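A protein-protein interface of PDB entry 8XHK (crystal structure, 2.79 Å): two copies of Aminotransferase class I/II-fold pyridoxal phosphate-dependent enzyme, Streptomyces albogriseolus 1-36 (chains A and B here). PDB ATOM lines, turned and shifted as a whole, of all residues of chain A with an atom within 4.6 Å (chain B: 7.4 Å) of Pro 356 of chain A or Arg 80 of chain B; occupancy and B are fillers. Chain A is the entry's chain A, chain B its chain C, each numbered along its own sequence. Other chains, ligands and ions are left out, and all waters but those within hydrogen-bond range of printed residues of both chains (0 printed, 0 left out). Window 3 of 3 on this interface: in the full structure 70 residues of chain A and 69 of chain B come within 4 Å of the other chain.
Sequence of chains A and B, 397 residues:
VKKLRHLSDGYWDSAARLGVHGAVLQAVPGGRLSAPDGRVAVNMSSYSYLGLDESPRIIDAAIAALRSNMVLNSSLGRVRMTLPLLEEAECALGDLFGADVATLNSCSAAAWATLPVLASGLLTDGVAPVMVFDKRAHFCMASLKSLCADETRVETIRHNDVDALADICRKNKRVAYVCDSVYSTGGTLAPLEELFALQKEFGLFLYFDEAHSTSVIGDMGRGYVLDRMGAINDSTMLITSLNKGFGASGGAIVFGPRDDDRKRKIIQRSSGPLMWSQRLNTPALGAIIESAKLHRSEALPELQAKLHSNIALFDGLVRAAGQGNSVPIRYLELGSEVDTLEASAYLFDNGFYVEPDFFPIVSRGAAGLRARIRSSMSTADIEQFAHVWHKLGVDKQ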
ATOM      1  N   VAL A  20      19.229 -24.516   5.844  1.00  0.00           N
ATOM      2  CA  VAL A  20      20.432 -24.612   5.025  1.00  0.00           C
ATOM      3  C   VAL A  20      21.554 -25.348   5.748  1.00  0.00           C
ATOM      4  O   VAL A  20      22.694 -25.352   5.275  1.00  0.00           O
ATOM      5  CB  VAL A  20      20.901 -23.224   4.566  1.00  0.00           C
ATOM      6  CG1 VAL A  20      19.796 -22.517   3.798  1.00  0.00           C
ATOM      7  CG2 VAL A  20      21.353 -22.393   5.760  1.00  0.00           C
ATOM      8  N   HIS A  21      21.259 -25.973   6.884  1.00  0.00           N
ATOM      9  CA  HIS A  21      22.284 -26.635   7.682  1.00  0.00           C
ATOM     10  C   HIS A  21      21.622 -27.738   8.489  1.00  0.00           C
ATOM     11  O   HIS A  21      20.664 -27.477   9.223  1.00  0.00           O
ATOM     12  CB  HIS A  21      22.983 -25.639   8.604  1.00  0.00           C
ATOM     13  CG  HIS A  21      24.435 -25.925   8.827  1.00  0.00           C
ATOM     14  ND1 HIS A  21      25.430 -25.357   8.061  1.00  0.00           N
ATOM     15  CD2 HIS A  21      25.060 -26.711   9.735  1.00  0.00           C
ATOM     16  CE1 HIS A  21      26.607 -25.779   8.488  1.00  0.00           C
ATOM     17  NE2 HIS A  21      26.410 -26.606   9.500  1.00  0.00           N
ATOM     18  N   GLY A  22      22.123 -28.961   8.345  1.00  0.00           N
ATOM     19  CA  GLY A  22      21.640 -30.059   9.156  1.00  0.00           C
ATOM     20  C   GLY A  22      20.231 -30.521   8.864  1.00  0.00           C
ATOM     21  O   GLY A  22      19.602 -31.131   9.732  1.00  0.00           O
ATOM     22  N   THR A 340      24.781 -14.235   4.891  1.00  0.00           N
ATOM     23  CA  THR A 340      25.187 -15.519   4.330  1.00  0.00           C
ATOM     24  C   THR A 340      24.065 -16.546   4.434  1.00  0.00           C
ATOM     25  O   THR A 340      23.702 -17.183   3.439  1.00  0.00           O
ATOM     26  CB  THR A 340      26.447 -16.025   5.034  1.00  0.00           C
ATOM     27  OG1 THR A 340      27.532 -15.123   4.781  1.00  0.00           O
ATOM     28  CG2 THR A 340      26.817 -17.407   4.527  1.00  0.00           C
ATOM     29  N   LEU A 341      23.499 -16.715   5.632  1.00  0.00           N
ATOM     30  CA  LEU A 341      22.439 -17.703   5.813  1.00  0.00           C
ATOM     31  C   LEU A 341      21.225 -17.376   4.954  1.00  0.00           C
ATOM     32  O   LEU A 341      20.556 -18.281   4.439  1.00  0.00           O
ATOM     33  CB  LEU A 341      22.042 -17.789   7.285  1.00  0.00           C
ATOM     34  CG  LEU A 341      23.125 -18.249   8.260  1.00  0.00           C
ATOM     35  CD1 LEU A 341      22.551 -18.382   9.659  1.00  0.00           C
ATOM     36  CD2 LEU A 341      23.736 -19.561   7.798  1.00  0.00           C
ATOM     37  N   SER A 344      21.977 -18.213   1.231  1.00  0.00           N
ATOM     38  CA  SER A 344      21.836 -19.645   0.996  1.00  0.00           C
ATOM     39  C   SER A 344      20.368 -20.048   0.941  1.00  0.00           C
ATOM     40  O   SER A 344      19.972 -20.863   0.099  1.00  0.00           O
ATOM     41  CB  SER A 344      22.574 -20.426   2.083  1.00  0.00           C
ATOM     42  OG  SER A 344      22.528 -21.822   1.838  1.00  0.00           O
ATOM     43  N   TYR A 353      21.690 -25.129  -4.087  1.00  0.00           N
ATOM     44  CA  TYR A 353      22.216 -25.170  -2.733  1.00  0.00           C
ATOM     45  C   TYR A 353      23.704 -24.855  -2.757  1.00  0.00           C
ATOM     46  O   TYR A 353      24.445 -25.374  -3.595  1.00  0.00           O
ATOM     47  CB  TYR A 353      21.990 -26.532  -2.071  1.00  0.00           C
ATOM     48  CG  TYR A 353      22.643 -26.619  -0.711  1.00  0.00           C
ATOM     49  CD1 TYR A 353      21.981 -26.179   0.426  1.00  0.00           C
ATOM     50  CD2 TYR A 353      23.931 -27.117  -0.567  1.00  0.00           C
ATOM     51  CE1 TYR A 353      22.579 -26.242   1.669  1.00  0.00           C
ATOM     52  CE2 TYR A 353      24.536 -27.175   0.664  1.00  0.00           C
ATOM     53  CZ  TYR A 353      23.857 -26.744   1.783  1.00  0.00           C
ATOM     54  OH  TYR A 353      24.460 -26.811   3.018  1.00  0.00           O
ATOM     55  N   VAL A 354      24.138 -24.012  -1.826  1.00  0.00           N
ATOM     56  CA  VAL A 354      25.550 -23.680  -1.724  1.00  0.00           C
ATOM     57  C   VAL A 354      26.067 -24.001  -0.326  1.00  0.00           C
ATOM     58  O   VAL A 354      25.793 -23.277   0.628  1.00  0.00           O
ATOM     59  CB  VAL A 354      25.805 -22.205  -2.077  1.00  0.00           C
ATOM     60  CG1 VAL A 354      27.293 -21.963  -2.255  1.00  0.00           C
ATOM     61  CG2 VAL A 354      25.047 -21.817  -3.338  1.00  0.00           C
ATOM     62  N   PRO A 356      26.942 -22.964   3.341  1.00  0.00           N
ATOM     63  CA  PRO A 356      27.393 -21.700   3.931  1.00  0.00           C
ATOM     64  C   PRO A 356      28.335 -21.897   5.116  1.00  0.00           C
ATOM     65  O   PRO A 356      28.094 -22.760   5.960  1.00  0.00           O
ATOM     66  CB  PRO A 356      26.086 -21.050   4.386  1.00  0.00           C
ATOM     67  CG  PRO A 356      25.211 -22.203   4.721  1.00  0.00           C
ATOM     68  CD  PRO A 356      25.565 -23.297   3.745  1.00  0.00           C
ATOM     69  N   ASP A 357      29.396 -21.099   5.173  1.00  0.00           N
ATOM     70  CA  ASP A 357      30.356 -21.140   6.265  1.00  0.00           C
ATOM     71  C   ASP A 357      30.185 -19.910   7.147  1.00  0.00           C
ATOM     72  O   ASP A 357      29.949 -18.807   6.648  1.00  0.00           O
ATOM     73  CB  ASP A 357      31.793 -21.213   5.736  1.00  0.00           C
ATOM     74  CG  ASP A 357      32.111 -22.553   5.097  1.00  0.00           C
ATOM     75  OD1 ASP A 357      31.273 -23.475   5.195  1.00  0.00           O
ATOM     76  OD2 ASP A 357      33.200 -22.685   4.494  1.00  0.00           O
ATOM     77  N   PHE A 358      30.300 -20.109   8.458  1.00  0.00           N
ATOM     78  CA  PHE A 358      30.167 -19.024   9.420  1.00  0.00           C
ATOM     79  C   PHE A 358      30.992 -19.362  10.656  1.00  0.00           C
ATOM     80  O   PHE A 358      31.618 -20.421  10.738  1.00  0.00           O
ATOM     81  CB  PHE A 358      28.695 -18.776   9.773  1.00  0.00           C
ATOM     82  CG  PHE A 358      27.916 -20.030  10.043  1.00  0.00           C
ATOM     83  CD1 PHE A 358      28.032 -20.687  11.257  1.00  0.00           C
ATOM     84  CD2 PHE A 358      27.062 -20.549   9.086  1.00  0.00           C
ATOM     85  CE1 PHE A 358      27.316 -21.843  11.508  1.00  0.00           C
ATOM     86  CE2 PHE A 358      26.341 -21.704   9.332  1.00  0.00           C
ATOM     87  CZ  PHE A 358      26.469 -22.352  10.544  1.00  0.00           C
ATOM     88  N   ILE A 361      33.361 -21.909  12.085  1.00  0.00           N
ATOM     89  CA  ILE A 361      34.061 -22.556  10.974  1.00  0.00           C
ATOM     90  C   ILE A 361      35.061 -21.588  10.351  1.00  0.00           C
ATOM     91  O   ILE A 361      36.218 -21.939  10.093  1.00  0.00           O
ATOM     92  CB  ILE A 361      33.058 -23.075   9.928  1.00  0.00           C
ATOM     93  CG1 ILE A 361      31.895 -23.797  10.610  1.00  0.00           C
ATOM     94  CG2 ILE A 361      33.755 -23.989   8.931  1.00  0.00           C
ATOM     95  CD1 ILE A 361      30.699 -24.015   9.703  1.00  0.00           C
ATOM     96  N   GLY A 368      30.607 -16.672   4.383  1.00  0.00           N
ATOM     97  CA  GLY A 368      30.253 -16.664   2.983  1.00  0.00           C
ATOM     98  C   GLY A 368      29.743 -18.012   2.529  1.00  0.00           C
ATOM     99  O   GLY A 368      29.408 -18.874   3.341  1.00  0.00           O
ATOM    100  N   LEU A 369      29.696 -18.182   1.212  1.00  0.00           N
ATOM    101  CA  LEU A 369      29.194 -19.397   0.588  1.00  0.00           C
ATOM    102  C   LEU A 369      30.347 -20.143  -0.066  1.00  0.00           C
ATOM    103  O   LEU A 369      31.104 -19.561  -0.850  1.00  0.00           O
ATOM    104  CB  LEU A 369      28.114 -19.069  -0.441  1.00  0.00           C
ATOM    105  CG  LEU A 369      26.877 -18.380   0.134  1.00  0.00           C
ATOM    106  CD1 LEU A 369      25.872 -18.069  -0.964  1.00  0.00           C
ATOM    107  CD2 LEU A 369      26.248 -19.236   1.218  1.00  0.00           C
ATOM    108  N   SER B  74      26.496 -40.800   2.078  1.00  0.00           N
ATOM    109  CA  SER B  74      25.317 -40.292   2.778  1.00  0.00           C
ATOM    110  C   SER B  74      25.491 -38.830   3.171  1.00  0.00           C
ATOM    111  O   SER B  74      25.071 -38.418   4.259  1.00  0.00           O
ATOM    112  CB  SER B  74      25.038 -41.152   4.005  1.00  0.00           C
ATOM    113  OG  SER B  74      26.094 -41.056   4.945  1.00  0.00           O
ATOM    114  N   SER B  75      26.100 -38.041   2.273  1.00  0.00           N
ATOM    115  CA  SER B  75      26.592 -36.678   2.487  1.00  0.00           C
ATOM    116  C   SER B  75      27.868 -36.646   3.318  1.00  0.00           C
ATOM    117  O   SER B  75      28.162 -35.634   3.965  1.00  0.00           O
ATOM    118  CB  SER B  75      25.539 -35.761   3.120  1.00  0.00           C
ATOM    119  OG  SER B  75      25.351 -36.073   4.489  1.00  0.00           O
ATOM    120  N   ARG B  78      31.241 -34.269   2.419  1.00  0.00           N
ATOM    121  CA  ARG B  78      30.473 -33.410   1.530  1.00  0.00           C
ATOM    122  C   ARG B  78      29.757 -32.326   2.316  1.00  0.00           C
ATOM    123  O   ARG B  78      30.392 -31.452   2.917  1.00  0.00           O
ATOM    124  CB  ARG B  78      29.453 -34.219   0.718  1.00  0.00           C
ATOM    125  CG  ARG B  78      29.889 -34.532  -0.706  1.00  0.00           C
ATOM    126  CD  ARG B  78      28.706 -34.653  -1.666  1.00  0.00           C
ATOM    127  NE  ARG B  78      27.805 -35.752  -1.336  1.00  0.00           N
ATOM    128  CZ  ARG B  78      26.572 -35.596  -0.874  1.00  0.00           C
ATOM    129  NH1 ARG B  78      26.054 -34.396  -0.673  1.00  0.00           N
ATOM    130  NH2 ARG B  78      25.836 -36.674  -0.614  1.00  0.00           N
ATOM    131  N   VAL B  79      28.435 -32.389   2.329  1.00  0.00           N
ATOM    132  CA  VAL B  79      27.623 -31.333   2.888  1.00  0.00           C
ATOM    133  C   VAL B  79      27.178 -31.717   4.293  1.00  0.00           C
ATOM    134  O   VAL B  79      27.118 -32.892   4.665  1.00  0.00           O
ATOM    135  CB  VAL B  79      26.415 -31.028   1.979  1.00  0.00           C
ATOM    136  CG1 VAL B  79      25.838 -29.685   2.329  1.00  0.00           C
ATOM    137  CG2 VAL B  79      26.836 -31.066   0.515  1.00  0.00           C
ATOM    138  N   ARG B  80      26.875 -30.694   5.092  1.00  0.00           N
ATOM    139  CA  ARG B  80      26.321 -30.858   6.428  1.00  0.00           C
ATOM    140  C   ARG B  80      24.907 -31.422   6.408  1.00  0.00           C
ATOM    141  O   ARG B  80      24.400 -31.819   7.462  1.00  0.00           O
ATOM    142  CB  ARG B  80      26.344 -29.519   7.173  1.00  0.00           C
ATOM    143  CG  ARG B  80      26.460 -28.273   6.284  1.00  0.00           C
ATOM    144  CD  ARG B  80      27.906 -27.971   5.876  1.00  0.00           C
ATOM    145  NE  ARG B  80      28.837 -28.059   6.996  1.00  0.00           N
ATOM    146  CZ  ARG B  80      29.539 -27.040   7.472  1.00  0.00           C
ATOM    147  NH1 ARG B  80      29.447 -25.830   6.943  1.00  0.00           N
ATOM    148  NH2 ARG B  80      30.360 -27.242   8.498  1.00  0.00           N
ATOM    149  N   MET B  81      24.265 -31.467   5.243  1.00  0.00           N
ATOM    150  CA  MET B  81      23.003 -32.171   5.102  1.00  0.00           C
ATOM    151  C   MET B  81      23.233 -33.670   5.281  1.00  0.00           C
ATOM    152  O   MET B  81      24.353 -34.132   5.506  1.00  0.00           O
ATOM    153  CB  MET B  81      22.369 -31.871   3.747  1.00  0.00           C
ATOM    154  CG  MET B  81      22.551 -30.436   3.290  1.00  0.00           C
ATOM    155  SD  MET B  81      21.944 -29.231   4.480  1.00  0.00           S
ATOM    156  CE  MET B  81      20.182 -29.369   4.212  1.00  0.00           C
ATOM    157  N   THR B  82      22.157 -34.444   5.177  1.00  0.00           N
ATOM    158  CA  THR B  82      22.249 -35.882   5.378  1.00  0.00           C
ATOM    159  C   THR B  82      21.104 -36.572   4.655  1.00  0.00           C
ATOM    160  O   THR B  82      20.010 -36.016   4.520  1.00  0.00           O
ATOM    161  CB  THR B  82      22.224 -36.245   6.867  1.00  0.00           C
ATOM    162  OG1 THR B  82      22.185 -37.669   7.011  1.00  0.00           O
ATOM    163  CG2 THR B  82      21.008 -35.638   7.549  1.00  0.00           C
ATOM    164  N   MET B 275      32.452 -34.126  12.723  1.00  0.00           N
ATOM    165  CA  MET B 275      32.241 -32.972  11.858  1.00  0.00           C
ATOM    166  C   MET B 275      33.032 -33.044  10.557  1.00  0.00           C
ATOM    167  O   MET B 275      32.459 -32.865   9.478  1.00  0.00           O
ATOM    168  CB  MET B 275      32.603 -31.686  12.612  1.00  0.00           C
ATOM    169  CG  MET B 275      32.762 -30.470  11.715  1.00  0.00           C
ATOM    170  SD  MET B 275      32.914 -28.937  12.646  1.00  0.00           S
ATOM    171  CE  MET B 275      31.469 -28.063  12.056  1.00  0.00           C
ATOM    172  N   ARG B 279      30.939 -39.752   7.182  1.00  0.00           N
ATOM    173  CA  ARG B 279      29.905 -40.643   7.675  1.00  0.00           C
ATOM    174  C   ARG B 279      29.969 -41.988   6.949  1.00  0.00           C
ATOM    175  O   ARG B 279      30.785 -42.210   6.051  1.00  0.00           O
ATOM    176  CB  ARG B 279      28.536 -39.987   7.506  1.00  0.00           C
ATOM    177  CG  ARG B 279      28.266 -38.852   8.492  1.00  0.00           C
ATOM    178  CD  ARG B 279      27.873 -37.555   7.793  1.00  0.00           C
ATOM    179  NE  ARG B 279      27.406 -36.544   8.738  1.00  0.00           N
ATOM    180  CZ  ARG B 279      27.131 -35.286   8.422  1.00  0.00           C
ATOM    181  NH1 ARG B 279      27.286 -34.832   7.189  1.00  0.00           N
ATOM    182  NH2 ARG B 279      26.690 -34.461   9.368  1.00  0.00           N
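Of the printed residues of chain B, His 21 of chain A touches Arg 80 (3.2 Å). Printed residues of chain B within 4 Å of Tyr 353 of chain A: Val 79 and Met 81. Of the printed residues of chain B, Asp 357 of chain A touches Arg 80 (3.5 Å). Phe 358 of chain A touches none of the printed residues of chain B. Printed residues of chain B within 4 Å of Ile 361 of chain A: Arg 80. Of chain A, only His 21 (3.2 Å), Gly 22 (3.7 Å), Pro 356 (3.5 Å), Asp 357 (3.5 Å) and Ile 361 (3.5 Å) come within 4 Å of Arg 80 of chain B. Printed residues of chain A within 4 Å of Met 81 of chain B: Gly 22 and Tyr 353. The nearest residue of chain A that does not touch Arg 80 of chain B is Tyr 353 of chain A (4.1 Å). The nearest printed residue of chain B that does not touch His 21 of chain A is Met 81 of chain B (4.1 Å).
No position is printed for both chains. Of the 8 pairs that touch across the chains among the printed residues, none has its exchanged pair printed and touching as well.
NH1 of Arg 80 of chain B touches CE1 of His 21 of chain A, 3.2 Å away. O of Arg 80 of chain B touches CA of Gly 22 of chain A, 3.7 Å away. Gly 22 of chain A touches Met 81 of chain B. Val 79 of chain B touches Tyr 353 of chain A (CG1 to OH, 3.3 Å). CD1 of Ile 361 of chain A touches NH2 of Arg 80 of chain B (3.5 Å).
The backbone carbonyl oxygen (O) of Pro 356 of chain A is in hydrogen-bond range of the guanidinium group (NH1) of Arg 80 of chain B, at 3.5 Å. The guanidinium group of Arg 80 of chain B lies within salt-bridge range of the side-chain carboxylate of Asp 357 of chain A (3.5 Å). SD of Met 81 of chain B sits at hydrogen-bond distance from OH of Tyr 353 of chain A (3.8 Å).
OG of Ser 75 of chain B sits at hydrogen-bond distance from O of Met 81 of chain B (2.4 Å). The backbone carbonyl oxygen (O) of Val 79 of chain B lies within hydrogen-bond range of the guanidinium group (NH1) of Arg 279 of chain B (3.2 Å). The backbone carbonyl oxygen (O) of Met 81 of chain B sits at hydrogen-bond distance from the guanidinium group (NH1) of Arg 279 of chain B (3.5 Å). O of Val 20 of chain A lies within hydrogen-bond range of OH of Tyr 353 of chain A, 3.2 Å away. The backbone NH (N) of Asp 357 of chain A is in hydrogen-bond range of the backbone carbonyl oxygen (O) of Gly 368 of chain A (2.9 Å).
Hydrophobic or aromatic side chains of chain A that line the printed part of chain B: His 21, Tyr 353 and Ile 361. Of the 9 printed residues of chain B, 3 touch a printed residue of chain A. Hydrophobic or aromatic side chains of chain B that line the printed part of chain A: Val 79 and Met 81. Among the printed residues, Asp or Glu carboxylates within 4 Å of a Lys or Arg side-chain nitrogen of the other chain: Asp 357 of chain A with Arg 80 of chain B (3.5 Å).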
